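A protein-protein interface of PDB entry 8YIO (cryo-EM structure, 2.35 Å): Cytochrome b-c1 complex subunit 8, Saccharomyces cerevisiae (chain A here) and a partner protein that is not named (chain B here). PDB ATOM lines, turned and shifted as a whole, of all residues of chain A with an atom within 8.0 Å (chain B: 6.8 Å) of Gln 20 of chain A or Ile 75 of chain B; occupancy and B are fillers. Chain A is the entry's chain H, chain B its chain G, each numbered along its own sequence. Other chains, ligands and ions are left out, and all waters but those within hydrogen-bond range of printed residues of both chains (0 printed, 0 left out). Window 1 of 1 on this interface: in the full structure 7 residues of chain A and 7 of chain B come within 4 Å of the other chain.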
ATOM      1  N   GLY A  17     -11.995  16.646 -33.107  1.00  0.00           N
ATOM      2  CA  GLY A  17     -10.909  17.583 -33.242  1.00  0.00           C
ATOM      3  C   GLY A  17      -9.565  16.890 -33.141  1.00  0.00           C
ATOM      4  O   GLY A  17      -9.478  15.659 -33.165  1.00  0.00           O
ATOM      5  N   PRO A  18      -8.489  17.663 -33.031  1.00  0.00           N
ATOM      6  CA  PRO A  18      -7.168  17.062 -32.823  1.00  0.00           C
ATOM      7  C   PRO A  18      -7.007  16.564 -31.393  1.00  0.00           C
ATOM      8  O   PRO A  18      -7.809  16.850 -30.503  1.00  0.00           O
ATOM      9  CB  PRO A  18      -6.205  18.210 -33.130  1.00  0.00           C
ATOM     10  CG  PRO A  18      -6.982  19.436 -32.814  1.00  0.00           C
ATOM     11  CD  PRO A  18      -8.416  19.128 -33.160  1.00  0.00           C
ATOM     12  N   LYS A  19      -5.944  15.797 -31.183  1.00  0.00           N
ATOM     13  CA  LYS A  19      -5.638  15.276 -29.859  1.00  0.00           C
ATOM     14  C   LYS A  19      -5.009  16.357 -28.993  1.00  0.00           C
ATOM     15  O   LYS A  19      -4.123  17.092 -29.434  1.00  0.00           O
ATOM     16  CB  LYS A  19      -4.706  14.071 -29.962  1.00  0.00           C
ATOM     17  CG  LYS A  19      -5.397  12.815 -30.439  1.00  0.00           C
ATOM     18  CD  LYS A  19      -4.545  11.588 -30.206  1.00  0.00           C
ATOM     19  CE  LYS A  19      -5.306  10.326 -30.560  1.00  0.00           C
ATOM     20  NZ  LYS A  19      -4.792   9.146 -29.822  1.00  0.00           N
ATOM     21  N   GLN A  20      -5.476  16.454 -27.754  1.00  0.00           N
ATOM     22  CA  GLN A  20      -5.034  17.478 -26.822  1.00  0.00           C
ATOM     23  C   GLN A  20      -4.130  16.869 -25.760  1.00  0.00           C
ATOM     24  O   GLN A  20      -4.418  15.793 -25.229  1.00  0.00           O
ATOM     25  CB  GLN A  20      -6.228  18.163 -26.156  1.00  0.00           C
ATOM     26  CG  GLN A  20      -7.186  18.819 -27.124  1.00  0.00           C
ATOM     27  CD  GLN A  20      -8.275  19.597 -26.423  1.00  0.00           C
ATOM     28  OE1 GLN A  20      -8.101  20.040 -25.290  1.00  0.00           O
ATOM     29  NE2 GLN A  20      -9.407  19.767 -27.092  1.00  0.00           N
ATOM     30  N   LYS A  21      -3.046  17.572 -25.447  1.00  0.00           N
ATOM     31  CA  LYS A  21      -2.095  17.127 -24.440  1.00  0.00           C
ATOM     32  C   LYS A  21      -1.340  18.337 -23.915  1.00  0.00           C
ATOM     33  O   LYS A  21      -0.777  19.101 -24.700  1.00  0.00           O
ATOM     34  CB  LYS A  21      -1.124  16.095 -25.026  1.00  0.00           C
ATOM     35  CG  LYS A  21      -0.307  15.328 -24.007  1.00  0.00           C
ATOM     36  CD  LYS A  21       0.501  14.245 -24.690  1.00  0.00           C
ATOM     37  CE  LYS A  21       1.714  13.835 -23.875  1.00  0.00           C
ATOM     38  NZ  LYS A  21       1.370  13.003 -22.700  1.00  0.00           N
ATOM     39  N   GLY A  22      -1.343  18.516 -22.597  1.00  0.00           N
ATOM     40  CA  GLY A  22      -0.556  19.551 -21.963  1.00  0.00           C
ATOM     41  C   GLY A  22      -1.308  20.784 -21.508  1.00  0.00           C
ATOM     42  O   GLY A  22      -0.672  21.721 -21.023  1.00  0.00           O
ATOM     43  N   ILE A  23      -2.631  20.811 -21.633  1.00  0.00           N
ATOM     44  CA  ILE A  23      -3.441  21.978 -21.298  1.00  0.00           C
ATOM     45  C   ILE A  23      -4.222  21.689 -20.023  1.00  0.00           C
ATOM     46  O   ILE A  23      -4.921  20.674 -19.933  1.00  0.00           O
ATOM     47  CB  ILE A  23      -4.386  22.346 -22.456  1.00  0.00           C
ATOM     48  CG1 ILE A  23      -3.589  22.583 -23.739  1.00  0.00           C
ATOM     49  CG2 ILE A  23      -5.225  23.564 -22.108  1.00  0.00           C
ATOM     50  CD1 ILE A  23      -4.436  22.863 -24.947  1.00  0.00           C
ATOM     51  N   THR A  24      -4.103  22.580 -19.042  1.00  0.00           N
ATOM     52  CA  THR A  24      -4.837  22.503 -17.786  1.00  0.00           C
ATOM     53  C   THR A  24      -5.807  23.676 -17.689  1.00  0.00           C
ATOM     54  O   THR A  24      -5.478  24.793 -18.096  1.00  0.00           O
ATOM     55  CB  THR A  24      -3.870  22.510 -16.593  1.00  0.00           C
ATOM     56  OG1 THR A  24      -2.770  21.640 -16.868  1.00  0.00           O
ATOM     57  CG2 THR A  24      -4.552  22.038 -15.322  1.00  0.00           C
ATOM     58  N   SER A  25      -7.004  23.425 -17.158  1.00  0.00           N
ATOM     59  CA  SER A  25      -8.005  24.469 -16.973  1.00  0.00           C
ATOM     60  C   SER A  25      -8.489  24.508 -15.526  1.00  0.00           C
ATOM     61  O   SER A  25      -8.495  23.494 -14.827  1.00  0.00           O
ATOM     62  CB  SER A  25      -9.195  24.282 -17.923  1.00  0.00           C
ATOM     63  OG  SER A  25      -9.708  22.971 -17.860  1.00  0.00           O
ATOM     64  N   LEU B  42      -3.097  34.510 -32.448  1.00  0.00           N
ATOM     65  CA  LEU B  42      -3.193  33.576 -33.559  1.00  0.00           C
ATOM     66  C   LEU B  42      -2.170  33.899 -34.640  1.00  0.00           C
ATOM     67  O   LEU B  42      -1.798  35.055 -34.846  1.00  0.00           O
ATOM     68  CB  LEU B  42      -4.599  33.586 -34.170  1.00  0.00           C
ATOM     69  CG  LEU B  42      -5.774  33.114 -33.309  1.00  0.00           C
ATOM     70  CD1 LEU B  42      -7.090  33.668 -33.838  1.00  0.00           C
ATOM     71  CD2 LEU B  42      -5.829  31.592 -33.208  1.00  0.00           C
ATOM     72  N   TYR B  68       0.145  20.141 -30.997  1.00  0.00           N
ATOM     73  CA  TYR B  68      -0.271  20.474 -29.637  1.00  0.00           C
ATOM     74  C   TYR B  68      -0.296  21.981 -29.419  1.00  0.00           C
ATOM     75  O   TYR B  68      -1.175  22.496 -28.722  1.00  0.00           O
ATOM     76  CB  TYR B  68       0.651  19.809 -28.614  1.00  0.00           C
ATOM     77  CG  TYR B  68       0.568  18.301 -28.562  1.00  0.00           C
ATOM     78  CD1 TYR B  68      -0.644  17.646 -28.736  1.00  0.00           C
ATOM     79  CD2 TYR B  68       1.703  17.535 -28.329  1.00  0.00           C
ATOM     80  CE1 TYR B  68      -0.722  16.268 -28.690  1.00  0.00           C
ATOM     81  CE2 TYR B  68       1.638  16.159 -28.287  1.00  0.00           C
ATOM     82  CZ  TYR B  68       0.422  15.532 -28.464  1.00  0.00           C
ATOM     83  OH  TYR B  68       0.347  14.164 -28.415  1.00  0.00           O
ATOM     84  N   ARG B  70      -0.776  24.303 -31.769  1.00  0.00           N
ATOM     85  CA  ARG B  70      -1.868  24.878 -32.546  1.00  0.00           C
ATOM     86  C   ARG B  70      -3.196  24.755 -31.807  1.00  0.00           C
ATOM     87  O   ARG B  70      -4.027  25.668 -31.855  1.00  0.00           O
ATOM     88  CB  ARG B  70      -1.935  24.203 -33.921  1.00  0.00           C
ATOM     89  CG  ARG B  70      -3.108  24.608 -34.801  1.00  0.00           C
ATOM     90  CD  ARG B  70      -3.242  23.704 -36.016  1.00  0.00           C
ATOM     91  NE  ARG B  70      -4.405  24.039 -36.832  1.00  0.00           N
ATOM     92  CZ  ARG B  70      -5.583  23.430 -36.752  1.00  0.00           C
ATOM     93  NH1 ARG B  70      -6.579  23.812 -37.531  1.00  0.00           N
ATOM     94  NH2 ARG B  70      -5.770  22.442 -35.895  1.00  0.00           N
ATOM     95  N   ALA B  71      -3.399  23.644 -31.093  1.00  0.00           N
ATOM     96  CA  ALA B  71      -4.641  23.435 -30.357  1.00  0.00           C
ATOM     97  C   ALA B  71      -4.773  24.384 -29.170  1.00  0.00           C
ATOM     98  O   ALA B  71      -5.888  24.793 -28.834  1.00  0.00           O
ATOM     99  CB  ALA B  71      -4.733  21.985 -29.888  1.00  0.00           C
ATOM    100  N   TYR B  72      -3.658  24.760 -28.543  1.00  0.00           N
ATOM    101  CA  TYR B  72      -3.716  25.686 -27.417  1.00  0.00           C
ATOM    102  C   TYR B  72      -4.023  27.113 -27.875  1.00  0.00           C
ATOM    103  O   TYR B  72      -4.731  27.849 -27.179  1.00  0.00           O
ATOM    104  CB  TYR B  72      -2.407  25.639 -26.626  1.00  0.00           C
ATOM    105  CG  TYR B  72      -2.275  26.746 -25.611  1.00  0.00           C
ATOM    106  CD1 TYR B  72      -3.128  26.815 -24.518  1.00  0.00           C
ATOM    107  CD2 TYR B  72      -1.315  27.737 -25.758  1.00  0.00           C
ATOM    108  CE1 TYR B  72      -3.022  27.830 -23.594  1.00  0.00           C
ATOM    109  CE2 TYR B  72      -1.199  28.757 -24.837  1.00  0.00           C
ATOM    110  CZ  TYR B  72      -2.058  28.798 -23.758  1.00  0.00           C
ATOM    111  OH  TYR B  72      -1.952  29.807 -22.837  1.00  0.00           O
ATOM    112  N   ARG B  73      -3.514  27.517 -29.043  1.00  0.00           N
ATOM    113  CA  ARG B  73      -3.759  28.872 -29.539  1.00  0.00           C
ATOM    114  C   ARG B  73      -5.214  29.065 -29.956  1.00  0.00           C
ATOM    115  O   ARG B  73      -5.774  30.149 -29.776  1.00  0.00           O
ATOM    116  CB  ARG B  73      -2.817  29.189 -30.705  1.00  0.00           C
ATOM    117  CG  ARG B  73      -1.362  29.398 -30.311  1.00  0.00           C
ATOM    118  CD  ARG B  73      -0.512  29.965 -31.451  1.00  0.00           C
ATOM    119  NE  ARG B  73      -0.619  29.184 -32.680  1.00  0.00           N
ATOM    120  CZ  ARG B  73       0.243  28.246 -33.063  1.00  0.00           C
ATOM    121  NH1 ARG B  73       0.048  27.592 -34.196  1.00  0.00           N
ATOM    122  NH2 ARG B  73       1.297  27.960 -32.317  1.00  0.00           N
ATOM    123  N   ILE B  74      -5.841  28.022 -30.500  1.00  0.00           N
ATOM    124  CA  ILE B  74      -7.239  28.107 -30.913  1.00  0.00           C
ATOM    125  C   ILE B  74      -8.158  28.172 -29.694  1.00  0.00           C
ATOM    126  O   ILE B  74      -9.124  28.945 -29.670  1.00  0.00           O
ATOM    127  CB  ILE B  74      -7.570  26.923 -31.846  1.00  0.00           C
ATOM    128  CG1 ILE B  74      -6.958  27.158 -33.229  1.00  0.00           C
ATOM    129  CG2 ILE B  74      -9.073  26.685 -31.974  1.00  0.00           C
ATOM    130  CD1 ILE B  74      -7.106  25.993 -34.183  1.00  0.00           C
ATOM    131  N   ILE B  75      -7.845  27.399 -28.651  1.00  0.00           N
ATOM    132  CA  ILE B  75      -8.659  27.370 -27.439  1.00  0.00           C
ATOM    133  C   ILE B  75      -8.545  28.689 -26.676  1.00  0.00           C
ATOM    134  O   ILE B  75      -9.547  29.226 -26.189  1.00  0.00           O
ATOM    135  CB  ILE B  75      -8.260  26.153 -26.577  1.00  0.00           C
ATOM    136  CG1 ILE B  75      -8.842  24.870 -27.169  1.00  0.00           C
ATOM    137  CG2 ILE B  75      -8.702  26.294 -25.128  1.00  0.00           C
ATOM    138  CD1 ILE B  75      -8.285  23.612 -26.561  1.00  0.00           C
ATOM    139  N   ARG B  76      -7.332  29.246 -26.595  1.00  0.00           N
ATOM    140  CA  ARG B  76      -7.122  30.531 -25.929  1.00  0.00           C
ATOM    141  C   ARG B  76      -7.812  31.679 -26.669  1.00  0.00           C
ATOM    142  O   ARG B  76      -8.281  32.627 -26.033  1.00  0.00           O
ATOM    143  CB  ARG B  76      -5.617  30.798 -25.781  1.00  0.00           C
ATOM    144  CG  ARG B  76      -5.248  32.092 -25.054  1.00  0.00           C
ATOM    145  CD  ARG B  76      -3.743  32.310 -24.945  1.00  0.00           C
ATOM    146  NE  ARG B  76      -3.088  32.398 -26.244  1.00  0.00           N
ATOM    147  CZ  ARG B  76      -1.778  32.533 -26.418  1.00  0.00           C
ATOM    148  NH1 ARG B  76      -1.274  32.601 -27.639  1.00  0.00           N
ATOM    149  NH2 ARG B  76      -0.973  32.606 -25.373  1.00  0.00           N
ATOM    150  N   ALA B  77      -7.922  31.594 -27.997  1.00  0.00           N
ATOM    151  CA  ALA B  77      -8.599  32.640 -28.757  1.00  0.00           C
ATOM    152  C   ALA B  77     -10.115  32.590 -28.598  1.00  0.00           C
ATOM    153  O   ALA B  77     -10.771  33.631 -28.681  1.00  0.00           O
ATOM    154  CB  ALA B  77      -8.223  32.548 -30.237  1.00  0.00           C
ATOM    155  N   HIS B  78     -10.688  31.406 -28.368  1.00  0.00           N
ATOM    156  CA  HIS B  78     -12.124  31.313 -28.124  1.00  0.00           C
ATOM    157  C   HIS B  78     -12.497  31.874 -26.756  1.00  0.00           C
ATOM    158  O   HIS B  78     -13.551  32.497 -26.605  1.00  0.00           O
ATOM    159  CB  HIS B  78     -12.590  29.863 -28.243  1.00  0.00           C
ATOM    160  CG  HIS B  78     -12.896  29.433 -29.643  1.00  0.00           C
ATOM    161  ND1 HIS B  78     -12.230  28.403 -30.267  1.00  0.00           N
ATOM    162  CD2 HIS B  78     -13.801  29.891 -30.538  1.00  0.00           C
ATOM    163  CE1 HIS B  78     -12.709  28.246 -31.487  1.00  0.00           C
ATOM    164  NE2 HIS B  78     -13.663  29.137 -31.677  1.00  0.00           N
ATOM    165  N   GLN B  79     -11.646  31.657 -25.748  1.00  0.00           N
ATOM    166  CA  GLN B  79     -11.927  32.150 -24.403  1.00  0.00           C
ATOM    167  C   GLN B  79     -11.780  33.664 -24.318  1.00  0.00           C
ATOM    168  O   GLN B  79     -12.555  34.318 -23.616  1.00  0.00           O
ATOM    169  CB  GLN B  79     -11.012  31.449 -23.389  1.00  0.00           C
ATOM    170  CG  GLN B  79     -11.160  31.901 -21.935  1.00  0.00           C
ATOM    171  CD  GLN B  79     -12.489  31.505 -21.313  1.00  0.00           C
ATOM    172  OE1 GLN B  79     -13.052  30.466 -21.637  1.00  0.00           O
ATOM    173  NE2 GLN B  79     -12.989  32.335 -20.415  1.00  0.00           N
ATOM    174  N   THR B  80     -10.817  34.234 -25.043  1.00  0.00           N
ATOM    175  CA  THR B  80     -10.648  35.684 -25.075  1.00  0.00           C
ATOM    176  C   THR B  80     -11.800  36.364 -25.806  1.00  0.00           C
ATOM    177  O   THR B  80     -12.188  37.481 -25.450  1.00  0.00           O
ATOM    178  CB  THR B  80      -9.309  36.029 -25.738  1.00  0.00           C
ATOM    179  OG1 THR B  80      -8.286  35.180 -25.210  1.00  0.00           O
ATOM    180  CG2 THR B  80      -8.915  37.463 -25.472  1.00  0.00           C
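Lys 19 of chain A touches Tyr 68 of chain B (O to CE1, 3.6 Å).
Gln 20 of chain A touches Ile 75 of chain B.
Lys 21 of chain A touches Tyr 68 of chain B.
CD1 of Ile 23 of chain A touches CA of Tyr 72 of chain B, 3.8 Å away.
Pro 18 of chain A touches none of the printed residues of chain B.
Printed residues of chain B within 4 Å of Lys 19 of chain A: Tyr 68 (3.6 Å).
Of chain B, only Ile 75 comes within 4 Å of Gln 20 of chain A.
Printed residues of chain B within 4 Å of Lys 21 of chain A: Tyr 68 (3.7 Å).
Of the printed residues of chain A, Tyr 72 of chain B touches Ile 23.
Thr 80 of chain B touches none of the printed residues of chain A.
The nearest residue of chain B that does not touch Gln 20 of chain A is Tyr 68 of chain B (4.5 Å).
Printed residues of chain B that touch a printed residue of chain A: Tyr 68, Tyr 72 and Ile 75.
Printed residues of chain A that touch a printed residue of chain B: Lys 19, Gln 20, Lys 21 and Ile 23.
Hydrophobic or aromatic side chains of chain A within 4 Å of the printed part of chain B: Ile 23.
Among the printed residues, 4 pairs touch across the chains.
Among the printed residues, no Asp or Glu carboxylate lies within 4 Å of a Lys or Arg side-chain nitrogen of the other chain.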
